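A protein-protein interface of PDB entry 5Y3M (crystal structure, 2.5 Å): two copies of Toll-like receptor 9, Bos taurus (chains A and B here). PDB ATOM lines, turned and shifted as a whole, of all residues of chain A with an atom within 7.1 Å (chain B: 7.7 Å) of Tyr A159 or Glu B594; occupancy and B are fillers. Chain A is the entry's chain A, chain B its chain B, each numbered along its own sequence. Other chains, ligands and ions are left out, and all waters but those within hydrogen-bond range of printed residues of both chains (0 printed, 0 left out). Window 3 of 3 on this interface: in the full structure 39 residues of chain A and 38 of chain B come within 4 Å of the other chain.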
ATOM      1  N   GLY A  81      25.915  -5.962  -8.760  1.00  0.00           N
ATOM      2  CA  GLY A  81      25.622  -5.055  -7.644  1.00  0.00           C
ATOM      3  C   GLY A  81      26.526  -3.834  -7.538  1.00  0.00           C
ATOM      4  O   GLY A  81      26.096  -2.784  -7.057  1.00  0.00           O
ATOM      5  N   CYS A 157      29.848 -11.170  -0.177  1.00  0.00           N
ATOM      6  CA  CYS A 157      28.447 -11.480   0.142  1.00  0.00           C
ATOM      7  C   CYS A 157      27.815 -10.472   1.118  1.00  0.00           C
ATOM      8  O   CYS A 157      27.776 -10.688   2.334  1.00  0.00           O
ATOM      9  CB  CYS A 157      28.322 -12.914   0.667  1.00  0.00           C
ATOM     10  SG  CYS A 157      26.624 -13.529   0.634  1.00  0.00           S
ATOM     11  N   TYR A 158      27.333  -9.363   0.562  1.00  0.00           N
ATOM     12  CA  TYR A 158      26.602  -8.338   1.321  1.00  0.00           C
ATOM     13  C   TYR A 158      25.702  -7.524   0.374  1.00  0.00           C
ATOM     14  O   TYR A 158      25.667  -7.799  -0.817  1.00  0.00           O
ATOM     15  CB  TYR A 158      27.575  -7.451   2.119  1.00  0.00           C
ATOM     16  CG  TYR A 158      28.377  -6.443   1.311  1.00  0.00           C
ATOM     17  CD1 TYR A 158      29.266  -6.855   0.319  1.00  0.00           C
ATOM     18  CD2 TYR A 158      28.272  -5.076   1.568  1.00  0.00           C
ATOM     19  CE1 TYR A 158      30.004  -5.933  -0.412  1.00  0.00           C
ATOM     20  CE2 TYR A 158      29.009  -4.147   0.847  1.00  0.00           C
ATOM     21  CZ  TYR A 158      29.878  -4.582  -0.139  1.00  0.00           C
ATOM     22  OH  TYR A 158      30.607  -3.672  -0.863  1.00  0.00           O
ATOM     23  N   TYR A 159      24.969  -6.550   0.906  1.00  0.00           N
ATOM     24  CA  TYR A 159      23.984  -5.762   0.119  1.00  0.00           C
ATOM     25  C   TYR A 159      24.470  -5.195  -1.235  1.00  0.00           C
ATOM     26  O   TYR A 159      23.688  -5.118  -2.177  1.00  0.00           O
ATOM     27  CB  TYR A 159      23.359  -4.630   0.959  1.00  0.00           C
ATOM     28  CG  TYR A 159      24.337  -3.595   1.476  1.00  0.00           C
ATOM     29  CD1 TYR A 159      24.643  -2.454   0.737  1.00  0.00           C
ATOM     30  CD2 TYR A 159      24.938  -3.744   2.726  1.00  0.00           C
ATOM     31  CE1 TYR A 159      25.539  -1.503   1.216  1.00  0.00           C
ATOM     32  CE2 TYR A 159      25.836  -2.801   3.213  1.00  0.00           C
ATOM     33  CZ  TYR A 159      26.134  -1.683   2.452  1.00  0.00           C
ATOM     34  OH  TYR A 159      27.015  -0.739   2.914  1.00  0.00           O
ATOM     35  N   MET A 160      25.740  -4.811  -1.326  1.00  0.00           N
ATOM     36  CA  MET A 160      26.325  -4.266  -2.578  1.00  0.00           C
ATOM     37  C   MET A 160      26.842  -5.325  -3.556  1.00  0.00           C
ATOM     38  O   MET A 160      27.034  -5.025  -4.738  1.00  0.00           O
ATOM     39  CB  MET A 160      27.453  -3.275  -2.266  1.00  0.00           C
ATOM     40  CG  MET A 160      26.960  -1.931  -1.772  1.00  0.00           C
ATOM     41  SD  MET A 160      26.300  -0.836  -3.033  1.00  0.00           S
ATOM     42  CE  MET A 160      24.542  -1.142  -3.007  1.00  0.00           C
ATOM     43  N   ASN A 161      27.082  -6.542  -3.061  1.00  0.00           N
ATOM     44  CA  ASN A 161      27.583  -7.657  -3.877  1.00  0.00           C
ATOM     45  C   ASN A 161      26.997  -8.955  -3.310  1.00  0.00           C
ATOM     46  O   ASN A 161      27.699  -9.734  -2.665  1.00  0.00           O
ATOM     47  CB  ASN A 161      29.120  -7.660  -3.862  1.00  0.00           C
ATOM     48  CG  ASN A 161      29.727  -8.612  -4.883  1.00  0.00           C
ATOM     49  OD1 ASN A 161      29.143  -8.879  -5.931  1.00  0.00           O
ATOM     50  ND2 ASN A 161      30.923  -9.104  -4.589  1.00  0.00           N
ATOM     51  N   PRO A 162      25.683  -9.170  -3.523  1.00  0.00           N
ATOM     52  CA  PRO A 162      24.966 -10.217  -2.794  1.00  0.00           C
ATOM     53  C   PRO A 162      25.232 -11.641  -3.265  1.00  0.00           C
ATOM     54  O   PRO A 162      25.535 -11.873  -4.437  1.00  0.00           O
ATOM     55  CB  PRO A 162      23.494  -9.857  -3.019  1.00  0.00           C
ATOM     56  CG  PRO A 162      23.477  -9.131  -4.311  1.00  0.00           C
ATOM     57  CD  PRO A 162      24.772  -8.377  -4.375  1.00  0.00           C
ATOM     58  N   CYS A 163      25.127 -12.571  -2.320  1.00  0.00           N
ATOM     59  CA  CYS A 163      25.104 -13.998  -2.606  1.00  0.00           C
ATOM     60  C   CYS A 163      23.927 -14.610  -1.827  1.00  0.00           C
ATOM     61  O   CYS A 163      23.463 -14.015  -0.854  1.00  0.00           O
ATOM     62  CB  CYS A 163      26.456 -14.646  -2.256  1.00  0.00           C
ATOM     63  SG  CYS A 163      26.711 -15.203  -0.551  1.00  0.00           S
ATOM     64  N   TYR A 187      32.564  -8.352   5.252  1.00  0.00           N
ATOM     65  CA  TYR A 187      31.353  -8.294   4.414  1.00  0.00           C
ATOM     66  C   TYR A 187      31.153  -9.553   3.548  1.00  0.00           C
ATOM     67  O   TYR A 187      30.892  -9.461   2.340  1.00  0.00           O
ATOM     68  CB  TYR A 187      31.372  -7.028   3.541  1.00  0.00           C
ATOM     69  CG  TYR A 187      31.236  -5.737   4.311  1.00  0.00           C
ATOM     70  CD1 TYR A 187      29.981  -5.256   4.690  1.00  0.00           C
ATOM     71  CD2 TYR A 187      32.357  -4.972   4.638  1.00  0.00           C
ATOM     72  CE1 TYR A 187      29.848  -4.061   5.390  1.00  0.00           C
ATOM     73  CE2 TYR A 187      32.235  -3.775   5.335  1.00  0.00           C
ATOM     74  CZ  TYR A 187      30.981  -3.325   5.706  1.00  0.00           C
ATOM     75  OH  TYR A 187      30.860  -2.142   6.402  1.00  0.00           O
ATOM     76  N   ARG A 235      25.031  -6.230  15.291  1.00  0.00           N
ATOM     77  CA  ARG A 235      25.037  -4.776  15.302  1.00  0.00           C
ATOM     78  C   ARG A 235      23.804  -4.162  15.943  1.00  0.00           C
ATOM     79  O   ARG A 235      22.798  -4.834  16.157  1.00  0.00           O
ATOM     80  CB  ARG A 235      25.122  -4.257  13.864  1.00  0.00           C
ATOM     81  CG  ARG A 235      26.289  -4.790  13.044  1.00  0.00           C
ATOM     82  CD  ARG A 235      26.243  -4.264  11.615  1.00  0.00           C
ATOM     83  NE  ARG A 235      26.241  -2.798  11.565  1.00  0.00           N
ATOM     84  CZ  ARG A 235      26.041  -2.061  10.475  1.00  0.00           C
ATOM     85  NH1 ARG A 235      25.830  -2.630   9.293  1.00  0.00           N
ATOM     86  NH2 ARG A 235      26.060  -0.735  10.567  1.00  0.00           N
ATOM     87  N   ARG A 241      23.978   3.450   9.037  1.00  0.00           N
ATOM     88  CA  ARG A 241      23.669   4.248   7.843  1.00  0.00           C
ATOM     89  C   ARG A 241      23.430   3.402   6.593  1.00  0.00           C
ATOM     90  O   ARG A 241      23.001   3.927   5.571  1.00  0.00           O
ATOM     91  CB  ARG A 241      24.751   5.294   7.575  1.00  0.00           C
ATOM     92  CG  ARG A 241      26.092   4.791   7.058  1.00  0.00           C
ATOM     93  CD  ARG A 241      26.749   5.803   6.133  1.00  0.00           C
ATOM     94  NE  ARG A 241      28.190   5.562   6.016  1.00  0.00           N
ATOM     95  CZ  ARG A 241      28.768   4.547   5.356  1.00  0.00           C
ATOM     96  NH1 ARG A 241      28.045   3.626   4.706  1.00  0.00           N
ATOM     97  NH2 ARG A 241      30.102   4.457   5.344  1.00  0.00           N
ATOM     98  N   ASN A 242      23.719   2.106   6.693  1.00  0.00           N
ATOM     99  CA  ASN A 242      23.634   1.169   5.574  1.00  0.00           C
ATOM    100  C   ASN A 242      22.678   0.028   5.950  1.00  0.00           C
ATOM    101  O   ASN A 242      22.196  -0.014   7.084  1.00  0.00           O
ATOM    102  CB  ASN A 242      25.046   0.654   5.198  1.00  0.00           C
ATOM    103  CG  ASN A 242      25.744  -0.082   6.328  1.00  0.00           C
ATOM    104  OD1 ASN A 242      25.348  -0.011   7.492  1.00  0.00           O
ATOM    105  ND2 ASN A 242      26.806  -0.790   5.983  1.00  0.00           N
ATOM    106  N   PRO A 243      22.371  -0.882   4.999  1.00  0.00           N
ATOM    107  CA  PRO A 243      21.572  -2.053   5.366  1.00  0.00           C
ATOM    108  C   PRO A 243      22.218  -2.865   6.487  1.00  0.00           C
ATOM    109  O   PRO A 243      23.435  -3.028   6.513  1.00  0.00           O
ATOM    110  CB  PRO A 243      21.511  -2.855   4.064  1.00  0.00           C
ATOM    111  CG  PRO A 243      21.559  -1.808   3.012  1.00  0.00           C
ATOM    112  CD  PRO A 243      22.525  -0.780   3.536  1.00  0.00           C
ATOM    113  N   CYS A 244      21.381  -3.365   7.390  1.00  0.00           N
ATOM    114  CA  CYS A 244      21.824  -3.860   8.684  1.00  0.00           C
ATOM    115  C   CYS A 244      20.821  -4.866   9.244  1.00  0.00           C
ATOM    116  O   CYS A 244      19.620  -4.603   9.246  1.00  0.00           O
ATOM    117  CB  CYS A 244      21.962  -2.664   9.639  1.00  0.00           C
ATOM    118  SG  CYS A 244      22.510  -3.038  11.319  1.00  0.00           S
ATOM    119  N   HIS B 566      22.773  13.384   3.240  1.00  0.00           N
ATOM    120  CA  HIS B 566      23.539  12.297   2.630  1.00  0.00           C
ATOM    121  C   HIS B 566      23.455  10.931   3.329  1.00  0.00           C
ATOM    122  O   HIS B 566      23.654   9.913   2.673  1.00  0.00           O
ATOM    123  CB  HIS B 566      25.003  12.723   2.482  1.00  0.00           C
ATOM    124  CG  HIS B 566      25.754  12.820   3.774  1.00  0.00           C
ATOM    125  ND1 HIS B 566      25.720  13.942   4.576  1.00  0.00           N
ATOM    126  CD2 HIS B 566      26.578  11.943   4.391  1.00  0.00           C
ATOM    127  CE1 HIS B 566      26.478  13.745   5.639  1.00  0.00           C
ATOM    128  NE2 HIS B 566      27.017  12.542   5.547  1.00  0.00           N
ATOM    129  N   SER B 567      23.195  10.897   4.638  1.00  0.00           N
ATOM    130  CA  SER B 567      23.074   9.636   5.371  1.00  0.00           C
ATOM    131  C   SER B 567      22.278   9.765   6.667  1.00  0.00           C
ATOM    132  O   SER B 567      22.064  10.860   7.167  1.00  0.00           O
ATOM    133  CB  SER B 567      24.468   9.054   5.675  1.00  0.00           C
ATOM    134  OG  SER B 567      25.160   9.809   6.660  1.00  0.00           O
ATOM    135  N   ARG B 568      21.855   8.616   7.191  1.00  0.00           N
ATOM    136  CA  ARG B 568      21.146   8.510   8.468  1.00  0.00           C
ATOM    137  C   ARG B 568      19.932   9.434   8.544  1.00  0.00           C
ATOM    138  O   ARG B 568      19.868  10.366   9.350  1.00  0.00           O
ATOM    139  CB  ARG B 568      22.101   8.750   9.637  1.00  0.00           C
ATOM    140  CG  ARG B 568      23.197   7.702   9.733  1.00  0.00           C
ATOM    141  CD  ARG B 568      23.954   7.812  11.039  1.00  0.00           C
ATOM    142  NE  ARG B 568      24.811   6.652  11.265  1.00  0.00           N
ATOM    143  CZ  ARG B 568      26.073   6.510  10.844  1.00  0.00           C
ATOM    144  NH1 ARG B 568      26.694   7.459  10.143  1.00  0.00           N
ATOM    145  NH2 ARG B 568      26.727   5.391  11.139  1.00  0.00           N
ATOM    146  N   LEU B 588      21.702  12.903  -2.832  1.00  0.00           N
ATOM    147  CA  LEU B 588      20.867  11.771  -3.205  1.00  0.00           C
ATOM    148  C   LEU B 588      21.745  10.665  -3.800  1.00  0.00           C
ATOM    149  O   LEU B 588      21.417   9.484  -3.691  1.00  0.00           O
ATOM    150  CB  LEU B 588      19.792  12.228  -4.196  1.00  0.00           C
ATOM    151  CG  LEU B 588      18.540  11.390  -4.429  1.00  0.00           C
ATOM    152  CD1 LEU B 588      17.780  11.108  -3.146  1.00  0.00           C
ATOM    153  CD2 LEU B 588      17.651  12.144  -5.400  1.00  0.00           C
ATOM    154  N   SER B 589      22.857  11.067  -4.419  1.00  0.00           N
ATOM    155  CA  SER B 589      23.912  10.160  -4.875  1.00  0.00           C
ATOM    156  C   SER B 589      24.383   9.193  -3.793  1.00  0.00           C
ATOM    157  O   SER B 589      24.385   7.978  -4.010  1.00  0.00           O
ATOM    158  CB  SER B 589      25.103  10.975  -5.380  1.00  0.00           C
ATOM    159  OG  SER B 589      26.164  10.150  -5.807  1.00  0.00           O
ATOM    160  N   GLN B 590      24.781   9.735  -2.644  1.00  0.00           N
ATOM    161  CA  GLN B 590      25.187   8.906  -1.491  1.00  0.00           C
ATOM    162  C   GLN B 590      24.038   8.046  -0.964  1.00  0.00           C
ATOM    163  O   GLN B 590      24.236   6.879  -0.643  1.00  0.00           O
ATOM    164  CB  GLN B 590      25.738   9.754  -0.335  1.00  0.00           C
ATOM    165  CG  GLN B 590      27.185  10.197  -0.493  1.00  0.00           C
ATOM    166  CD  GLN B 590      27.751  10.819   0.776  1.00  0.00           C
ATOM    167  OE1 GLN B 590      28.221  11.958   0.766  1.00  0.00           O
ATOM    168  NE2 GLN B 590      27.692  10.078   1.880  1.00  0.00           N
ATOM    169  N   MET B 591      22.847   8.635  -0.883  1.00  0.00           N
ATOM    170  CA  MET B 591      21.667   7.935  -0.384  1.00  0.00           C
ATOM    171  C   MET B 591      21.320   6.733  -1.257  1.00  0.00           C
ATOM    172  O   MET B 591      21.165   5.621  -0.755  1.00  0.00           O
ATOM    173  CB  MET B 591      20.474   8.885  -0.304  1.00  0.00           C
ATOM    174  CG  MET B 591      20.610   9.958   0.767  1.00  0.00           C
ATOM    175  SD  MET B 591      19.395  11.282   0.584  1.00  0.00           S
ATOM    176  CE  MET B 591      17.898  10.401   0.985  1.00  0.00           C
ATOM    177  N   TRP B 592      21.232   6.954  -2.565  1.00  0.00           N
ATOM    178  CA  TRP B 592      20.922   5.878  -3.514  1.00  0.00           C
ATOM    179  C   TRP B 592      22.055   4.862  -3.694  1.00  0.00           C
ATOM    180  O   TRP B 592      21.822   3.781  -4.220  1.00  0.00           O
ATOM    181  CB  TRP B 592      20.463   6.442  -4.874  1.00  0.00           C
ATOM    182  CG  TRP B 592      19.020   6.935  -4.899  1.00  0.00           C
ATOM    183  CD1 TRP B 592      18.000   6.588  -4.041  1.00  0.00           C
ATOM    184  CD2 TRP B 592      18.438   7.826  -5.859  1.00  0.00           C
ATOM    185  NE1 TRP B 592      16.837   7.226  -4.399  1.00  0.00           N
ATOM    186  CE2 TRP B 592      17.074   7.989  -5.510  1.00  0.00           C
ATOM    187  CE3 TRP B 592      18.938   8.509  -6.973  1.00  0.00           C
ATOM    188  CZ2 TRP B 592      16.205   8.809  -6.237  1.00  0.00           C
ATOM    189  CZ3 TRP B 592      18.076   9.327  -7.696  1.00  0.00           C
ATOM    190  CH2 TRP B 592      16.721   9.470  -7.324  1.00  0.00           C
ATOM    191  N   ALA B 593      23.265   5.206  -3.256  1.00  0.00           N
ATOM    192  CA  ALA B 593      24.372   4.251  -3.165  1.00  0.00           C
ATOM    193  C   ALA B 593      24.338   3.319  -1.935  1.00  0.00           C
ATOM    194  O   ALA B 593      25.144   2.391  -1.872  1.00  0.00           O
ATOM    195  CB  ALA B 593      25.701   4.999  -3.215  1.00  0.00           C
ATOM    196  N   GLU B 594      23.436   3.553  -0.973  1.00  0.00           N
ATOM    197  CA  GLU B 594      23.304   2.692   0.234  1.00  0.00           C
ATOM    198  C   GLU B 594      22.299   1.562   0.027  1.00  0.00           C
ATOM    199  O   GLU B 594      21.284   1.471   0.725  1.00  0.00           O
ATOM    200  CB  GLU B 594      22.873   3.506   1.459  1.00  0.00           C
ATOM    201  CG  GLU B 594      23.876   4.526   1.951  1.00  0.00           C
ATOM    202  CD  GLU B 594      25.091   3.939   2.648  1.00  0.00           C
ATOM    203  OE1 GLU B 594      25.209   2.698   2.758  1.00  0.00           O
ATOM    204  OE2 GLU B 594      25.947   4.745   3.060  1.00  0.00           O
ATOM    205  N   GLY B 595      22.596   0.695  -0.930  1.00  0.00           N
ATOM    206  CA  GLY B 595      21.686  -0.380  -1.299  1.00  0.00           C
ATOM    207  C   GLY B 595      20.356   0.198  -1.735  1.00  0.00           C
ATOM    208  O   GLY B 595      20.312   1.174  -2.486  1.00  0.00           O
ATOM    209  N   ASP B 596      19.282  -0.389  -1.223  1.00  0.00           N
ATOM    210  CA  ASP B 596      17.917   0.025  -1.547  1.00  0.00           C
ATOM    211  C   ASP B 596      17.208   0.695  -0.358  1.00  0.00           C
ATOM    212  O   ASP B 596      15.982   0.701  -0.289  1.00  0.00           O
ATOM    213  CB  ASP B 596      17.123  -1.191  -2.064  1.00  0.00           C
ATOM    214  CG  ASP B 596      17.677  -1.743  -3.396  1.00  0.00           C
ATOM    215  OD1 ASP B 596      18.048  -0.947  -4.304  1.00  0.00           O
ATOM    216  OD2 ASP B 596      17.734  -2.986  -3.541  1.00  0.00           O
ATOM    217  N   LEU B 597      17.976   1.292   0.553  1.00  0.00           N
ATOM    218  CA  LEU B 597      17.400   1.966   1.724  1.00  0.00           C
ATOM    219  C   LEU B 597      16.537   3.155   1.327  1.00  0.00           C
ATOM    220  O   LEU B 597      15.438   3.325   1.848  1.00  0.00           O
ATOM    221  CB  LEU B 597      18.485   2.453   2.697  1.00  0.00           C
ATOM    222  CG  LEU B 597      19.231   1.448   3.582  1.00  0.00           C
ATOM    223  CD1 LEU B 597      20.045   2.215   4.611  1.00  0.00           C
ATOM    224  CD2 LEU B 597      18.317   0.456   4.282  1.00  0.00           C
ATOM    225  N   TYR B 598      17.040   3.964   0.403  1.00  0.00           N
ATOM    226  CA  TYR B 598      16.356   5.173  -0.027  1.00  0.00           C
ATOM    227  C   TYR B 598      15.760   5.046  -1.435  1.00  0.00           C
ATOM    228  O   TYR B 598      15.503   6.052  -2.099  1.00  0.00           O
ATOM    229  CB  TYR B 598      17.328   6.349   0.062  1.00  0.00           C
ATOM    230  CG  TYR B 598      17.922   6.530   1.440  1.00  0.00           C
ATOM    231  CD1 TYR B 598      17.228   7.202   2.437  1.00  0.00           C
ATOM    232  CD2 TYR B 598      19.180   6.025   1.748  1.00  0.00           C
ATOM    233  CE1 TYR B 598      17.775   7.375   3.702  1.00  0.00           C
ATOM    234  CE2 TYR B 598      19.737   6.188   3.006  1.00  0.00           C
ATOM    235  CZ  TYR B 598      19.034   6.865   3.981  1.00  0.00           C
ATOM    236  OH  TYR B 598      19.590   7.029   5.223  1.00  0.00           O
ATOM    237  N   LEU B 599      15.514   3.814  -1.872  1.00  0.00           N
ATOM    238  CA  LEU B 599      14.920   3.551  -3.186  1.00  0.00           C
ATOM    239  C   LEU B 599      13.535   4.195  -3.351  1.00  0.00           C
ATOM    240  O   LEU B 599      13.200   4.659  -4.439  1.00  0.00           O
ATOM    241  CB  LEU B 599      14.811   2.037  -3.410  1.00  0.00           C
ATOM    242  CG  LEU B 599      14.325   1.534  -4.775  1.00  0.00           C
ATOM    243  CD1 LEU B 599      15.379   1.782  -5.838  1.00  0.00           C
ATOM    244  CD2 LEU B 599      13.978   0.055  -4.714  1.00  0.00           C
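NH1 of Arg A241 is in salt-bridge range of OE2 of Glu B594 (2.9 Å).
SD of Met A160 sits close to O of Ala B593, 3.6 Å away.
The side-chain hydroxyl (OH) of Tyr A159 lies within hydrogen-bond range of the side-chain amide nitrogen (ND2) of Asn A242, 3.1 Å away.
NH1 of Arg A235 is in hydrogen-bond range of OD1 of Asn A242 (3.2 Å).
NE2 of His B566 lies close to OG of Ser B567 (3.5 Å).
OH of Tyr B598 sits at hydrogen-bond distance from N of Arg B568, 3.4 Å away.
The side-chain sulfur (SG) of Cys A163 forms a disulfide with the side-chain sulfur (SG) of Cys A157 (2.1 Å).
Glu B594 touches Tyr A159.
N of Gly B595 touches CE of Met A160, at 3.4 Å.
CD of Arg A241 touches CB of Ser B567, 3.998 Å away.
Arg B568 touches Arg A241.
Arg A241 touches Leu B597 (O to CD1, 3.5 Å).
Glu B594 touches Asn A242.
C of Asn A242 touches CD1 of Leu B597, 3.7 Å away.
Pro A243 touches Glu B594 (CD to O, 3.8 Å).
CD1 of Leu B597 touches N of Pro A243 (3.9 Å).
Tyr A159 touches just one residue of chain B: Glu B594 (3.9 Å).
Printed residues of chain B within 4 Å of Met A160: Ala B593 and Gly B595.
Printed residues of chain B within 4 Å of Arg A241: Ser B567, Arg B568, Glu B594 and Leu B597.
Printed residues of chain A within 4 Å of Ser B567: Arg A241.
Ser B589 touches none of the printed residues of chain A.
Cys A244 touches none of the printed residues of chain B.
The nearest residue of chain B that does not touch Tyr A159 is Gly B595 (4.1 Å).
Hydrophobic or aromatic side chains of chain A that line the printed part of chain B: Tyr A159, Met A160 and Pro A243.
Of the 15 printed residues of chain B, 6 touch a printed residue of chain A.
Among the printed residues, 11 pairs touch across the chains.
Among the printed residues, Asp or Glu carboxylates within 4 Å of a Lys or Arg side-chain nitrogen of the other chain: Arg A241 with Glu B594.
No position is printed for both chains.
Of the 11 pairs that touch across the chains among the printed residues, none has its exchanged pair printed and touching as well.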
